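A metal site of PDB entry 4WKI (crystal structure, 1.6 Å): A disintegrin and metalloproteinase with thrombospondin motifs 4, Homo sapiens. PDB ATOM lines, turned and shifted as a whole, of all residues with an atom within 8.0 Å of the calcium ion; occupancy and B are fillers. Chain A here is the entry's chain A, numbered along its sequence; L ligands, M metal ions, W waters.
The calcium ion is bound by O of Cys 115 (2.3 Å), OD1 of Asp 108 (2.3 Å), O of Thr 117 (2.3 Å), OE1 of Glu 137 (2.4 Å), water W1 (2.4 Å) and O of Leu 109 (2.4 Å).
Within 4 Å of the calcium ion: Asp 108, Leu 109, Cys 115, Thr 117 and Glu 137.
The nearest printed residue that does not touch the calcium ion is Asp 116 (4.1 Å).
An oxygen (O3) of the ligand lies within hydrogen-bond range of the backbone NH of Leu 118 (2.8 Å).
O3 of the ligand lies within hydrogen-bond range of N of Gly 119.
The backbone carbonyl oxygen (O) of Gly 119 lies within hydrogen-bond range of a nitrogen (N3) of the ligand (3.0 Å).
The side-chain sulfur of Cys 115 forms a disulfide with the side-chain sulfur of Cys 110 (2.0 Å).
The backbone NH (N) of Cys 110 is in hydrogen-bond range of the side-chain hydroxyl (OG1) of Thr 117.
N of Glu 137 lies within hydrogen-bond range of O of Leu 118, at 2.7 Å.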
ATOM      1  N   PRO A  71     -16.931  -2.373   0.788  1.00  0.00           N
ATOM      2  CA  PRO A  71     -16.901  -1.424   1.906  1.00  0.00           C
ATOM      3  C   PRO A  71     -15.653  -1.506   2.791  1.00  0.00           C
ATOM      4  O   PRO A  71     -15.147  -0.479   3.230  1.00  0.00           O
ATOM      5  CB  PRO A  71     -18.150  -1.781   2.727  1.00  0.00           C
ATOM      6  CG  PRO A  71     -19.056  -2.471   1.767  1.00  0.00           C
ATOM      7  CD  PRO A  71     -18.180  -3.169   0.768  1.00  0.00           C
ATOM      8  N   ALA A  73     -12.132  -1.341   3.570  1.00  0.00           N
ATOM      9  CA  ALA A  73     -10.932  -0.805   2.949  1.00  0.00           C
ATOM     10  C   ALA A  73      -9.782  -1.809   3.062  1.00  0.00           C
ATOM     11  O   ALA A  73      -9.019  -1.984   2.105  1.00  0.00           O
ATOM     12  CB  ALA A  73     -10.549   0.506   3.581  1.00  0.00           C
ATOM     13  N   ARG A 106     -15.013   4.660  -6.727  1.00  0.00           N
ATOM     14  CA  ARG A 106     -16.134   5.429  -6.184  1.00  0.00           C
ATOM     15  C   ARG A 106     -16.801   4.732  -4.986  1.00  0.00           C
ATOM     16  O   ARG A 106     -17.671   5.318  -4.355  1.00  0.00           O
ATOM     17  CB  ARG A 106     -17.191   5.691  -7.253  1.00  0.00           C
ATOM     18  CG  ARG A 106     -16.707   6.383  -8.507  1.00  0.00           C
ATOM     19  CD  ARG A 106     -16.472   7.862  -8.274  1.00  0.00           C
ATOM     20  NE  ARG A 106     -17.710   8.632  -8.269  1.00  0.00           N
ATOM     21  CZ  ARG A 106     -17.764   9.947  -8.160  1.00  0.00           C
ATOM     22  NH1 ARG A 106     -18.949  10.561  -8.176  1.00  0.00           N
ATOM     23  NH2 ARG A 106     -16.651  10.661  -8.015  1.00  0.00           N
ATOM     24  N   GLN A 107     -16.395   3.490  -4.687  1.00  0.00           N
ATOM     25  CA  GLN A 107     -16.869   2.773  -3.492  1.00  0.00           C
ATOM     26  C   GLN A 107     -16.589   3.568  -2.218  1.00  0.00           C
ATOM     27  O   GLN A 107     -15.478   4.051  -1.995  1.00  0.00           O
ATOM     28  CB  GLN A 107     -16.187   1.400  -3.379  1.00  0.00           C
ATOM     29  CG  GLN A 107     -16.487   0.635  -2.093  1.00  0.00           C
ATOM     30  CD  GLN A 107     -17.925   0.161  -2.011  1.00  0.00           C
ATOM     31  OE1 GLN A 107     -18.451  -0.416  -2.977  1.00  0.00           O
ATOM     32  NE2 GLN A 107     -18.585   0.408  -0.879  1.00  0.00           N
ATOM     33  N   ASP A 108     -17.602   3.708  -1.373  1.00  0.00           N
ATOM     34  CA  ASP A 108     -17.401   4.285  -0.049  1.00  0.00           C
ATOM     35  C   ASP A 108     -16.610   3.278   0.792  1.00  0.00           C
ATOM     36  O   ASP A 108     -17.130   2.241   1.209  1.00  0.00           O
ATOM     37  CB  ASP A 108     -18.757   4.623   0.599  1.00  0.00           C
ATOM     38  CG  ASP A 108     -18.616   5.312   1.942  1.00  0.00           C
ATOM     39  OD1 ASP A 108     -17.485   5.572   2.403  1.00  0.00           O
ATOM     40  OD2 ASP A 108     -19.670   5.604   2.553  1.00  0.00           O
ATOM     41  N   LEU A 109     -15.327   3.591   1.015  1.00  0.00           N
ATOM     42  CA  LEU A 109     -14.435   2.725   1.774  1.00  0.00           C
ATOM     43  C   LEU A 109     -14.646   2.955   3.252  1.00  0.00           C
ATOM     44  O   LEU A 109     -14.866   4.085   3.687  1.00  0.00           O
ATOM     45  CB  LEU A 109     -12.968   3.010   1.414  1.00  0.00           C
ATOM     46  CG  LEU A 109     -12.565   2.670  -0.030  1.00  0.00           C
ATOM     47  CD1 LEU A 109     -11.131   3.138  -0.299  1.00  0.00           C
ATOM     48  CD2 LEU A 109     -12.696   1.170  -0.286  1.00  0.00           C
ATOM     49  N   CYS A 110     -14.570   1.871   4.037  1.00  0.00           N
ATOM     50  CA  CYS A 110     -14.840   1.937   5.468  1.00  0.00           C
ATOM     51  C   CYS A 110     -13.777   1.243   6.300  1.00  0.00           C
ATOM     52  O   CYS A 110     -13.122   0.300   5.843  1.00  0.00           O
ATOM     53  CB  CYS A 110     -16.218   1.313   5.775  1.00  0.00           C
ATOM     54  SG  CYS A 110     -17.576   1.890   4.740  1.00  0.00           S
ATOM     55  N   GLY A 111     -13.622   1.731   7.527  1.00  0.00           N
ATOM     56  CA  GLY A 111     -12.813   1.073   8.543  1.00  0.00           C
ATOM     57  C   GLY A 111     -13.711   0.151   9.371  1.00  0.00           C
ATOM     58  O   GLY A 111     -14.827  -0.174   8.960  1.00  0.00           O
ATOM     59  N   THR A 114     -16.470   3.164  11.235  1.00  0.00           N
ATOM     60  CA  THR A 114     -17.149   4.146  10.376  1.00  0.00           C
ATOM     61  C   THR A 114     -16.635   4.066   8.944  1.00  0.00           C
ATOM     62  O   THR A 114     -15.665   3.359   8.641  1.00  0.00           O
ATOM     63  CB  THR A 114     -16.979   5.615  10.856  1.00  0.00           C
ATOM     64  OG1 THR A 114     -15.698   6.119  10.494  1.00  0.00           O
ATOM     65  CG2 THR A 114     -17.197   5.750  12.378  1.00  0.00           C
ATOM     66  N   CYS A 115     -17.308   4.815   8.085  1.00  0.00           N
ATOM     67  CA  CYS A 115     -16.967   4.912   6.682  1.00  0.00           C
ATOM     68  C   CYS A 115     -16.356   6.262   6.329  1.00  0.00           C
ATOM     69  O   CYS A 115     -16.310   6.625   5.162  1.00  0.00           O
ATOM     70  CB  CYS A 115     -18.197   4.636   5.828  1.00  0.00           C
ATOM     71  SG  CYS A 115     -18.774   2.925   6.016  1.00  0.00           S
ATOM     72  N   ASP A 116     -15.836   6.965   7.339  1.00  0.00           N
ATOM     73  CA  ASP A 116     -15.159   8.268   7.154  1.00  0.00           C
ATOM     74  C   ASP A 116     -13.833   8.112   6.378  1.00  0.00           C
ATOM     75  O   ASP A 116     -13.295   9.088   5.863  1.00  0.00           O
ATOM     76  CB  ASP A 116     -14.860   8.926   8.501  1.00  0.00           C
ATOM     77  CG  ASP A 116     -16.111   9.247   9.297  1.00  0.00           C
ATOM     78  OD1 ASP A 116     -17.230   9.193   8.741  1.00  0.00           O
ATOM     79  OD2 ASP A 116     -15.975   9.553  10.501  1.00  0.00           O
ATOM     80  N   THR A 117     -13.320   6.890   6.345  1.00  0.00           N
ATOM     81  CA  THR A 117     -12.039   6.632   5.674  1.00  0.00           C
ATOM     82  C   THR A 117     -12.145   6.996   4.175  1.00  0.00           C
ATOM     83  O   THR A 117     -13.178   6.805   3.539  1.00  0.00           O
ATOM     84  CB  THR A 117     -11.542   5.175   5.886  1.00  0.00           C
ATOM     85  OG1 THR A 117     -12.264   4.252   5.071  1.00  0.00           O
ATOM     86  CG2 THR A 117     -11.671   4.750   7.355  1.00  0.00           C
ATOM     87  N   LEU A 118     -11.068   7.557   3.633  1.00  0.00           N
ATOM     88  CA  LEU A 118     -11.005   7.878   2.196  1.00  0.00           C
ATOM     89  C   LEU A 118      -9.964   7.051   1.448  1.00  0.00           C
ATOM     90  O   LEU A 118      -9.811   7.182   0.240  1.00  0.00           O
ATOM     91  CB  LEU A 118     -10.743   9.374   1.975  1.00  0.00           C
ATOM     92  CG  LEU A 118     -11.939  10.267   2.380  1.00  0.00           C
ATOM     93  CD1 LEU A 118     -11.479  11.716   2.464  1.00  0.00           C
ATOM     94  CD2 LEU A 118     -13.064  10.087   1.382  1.00  0.00           C
ATOM     95  N   GLY A 119      -9.232   6.209   2.157  1.00  0.00           N
ATOM     96  CA  GLY A 119      -8.174   5.446   1.496  1.00  0.00           C
ATOM     97  C   GLY A 119      -7.399   4.583   2.451  1.00  0.00           C
ATOM     98  O   GLY A 119      -7.592   4.648   3.668  1.00  0.00           O
ATOM     99  N   GLU A 137     -10.585   6.404  -2.248  1.00  0.00           N
ATOM    100  CA  GLU A 137     -11.989   6.701  -2.517  1.00  0.00           C
ATOM    101  C   GLU A 137     -12.048   8.055  -3.210  1.00  0.00           C
ATOM    102  O   GLU A 137     -11.673   9.076  -2.618  1.00  0.00           O
ATOM    103  CB  GLU A 137     -12.779   6.739  -1.221  1.00  0.00           C
ATOM    104  CG  GLU A 137     -14.253   7.075  -1.404  1.00  0.00           C
ATOM    105  CD  GLU A 137     -15.006   7.175  -0.102  1.00  0.00           C
ATOM    106  OE1 GLU A 137     -14.717   6.382   0.822  1.00  0.00           O
ATOM    107  OE2 GLU A 137     -15.902   8.043   0.010  1.00  0.00           O
HETATM  108  C1  LIG L   1      -9.095   3.640   9.276  1.00  0.00           C
HETATM  109  C2  LIG L   1      -7.938   2.934   9.057  1.00  0.00           C
HETATM  110  C3  LIG L   1      -6.159  13.073   3.398  1.00  0.00           C
HETATM  111  C4  LIG L   1      -7.304  10.773   3.964  1.00  0.00           C
HETATM  112  C5  LIG L   1      -8.213   7.367   7.512  1.00  0.00           C
HETATM  113  C6  LIG L   1      -6.202  11.924   5.493  1.00  0.00           C
HETATM  114  C7  LIG L   1      -7.799   4.985   8.207  1.00  0.00           C
HETATM  115  C8  LIG L   1      -5.423   6.333   6.059  1.00  0.00           C
HETATM  116  C9  LIG L   1      -7.255   6.189   7.519  1.00  0.00           C
HETATM  117  C10 LIG L   1      -5.786   3.426   7.976  1.00  0.00           C
HETATM  118  C11 LIG L   1      -5.091  13.933   5.392  1.00  0.00           C
HETATM  119  C12 LIG L   1      -5.475  12.869   6.169  1.00  0.00           C
HETATM  120  C13 LIG L   1      -5.419  14.034   4.065  1.00  0.00           C
HETATM  121  C14 LIG L   1      -6.567  11.971   4.165  1.00  0.00           C
HETATM  122  C15 LIG L   1      -7.338  10.098   5.165  1.00  0.00           C
HETATM  123  C16 LIG L   1      -6.015   6.654   8.226  1.00  0.00           C
HETATM  124  C17 LIG L   1      -7.915   8.864   5.591  1.00  0.00           C
HETATM  125  N1  LIG L   1      -8.996   4.902   8.750  1.00  0.00           N
HETATM  126  N2  LIG L   1      -5.039   6.773   7.285  1.00  0.00           N
HETATM  127  N3  LIG L   1      -6.721   5.889   6.202  1.00  0.00           N
HETATM  128  N4  LIG L   1      -7.626   8.553   6.906  1.00  0.00           N
HETATM  129  N5  LIG L   1      -7.128   3.801   8.378  1.00  0.00           N
HETATM  130  O1  LIG L   1      -5.946   6.905   9.417  1.00  0.00           O
HETATM  131  O2  LIG L   1      -4.733   6.337   5.048  1.00  0.00           O
HETATM  132  O3  LIG L   1      -8.569   8.143   4.836  1.00  0.00           O
HETATM  133  O4  LIG L   1      -6.659  10.813   6.105  1.00  0.00           O
HETATM  134 CL1  LIG L   1      -4.832  15.461   3.287  1.00  0.00          CL
HETATM  135 CA    CA M   1     -15.403   6.329   3.072  1.00  0.00          CA
HETATM  136  O   HOH W   1     -16.265   8.517   2.730  1.00  0.00           O
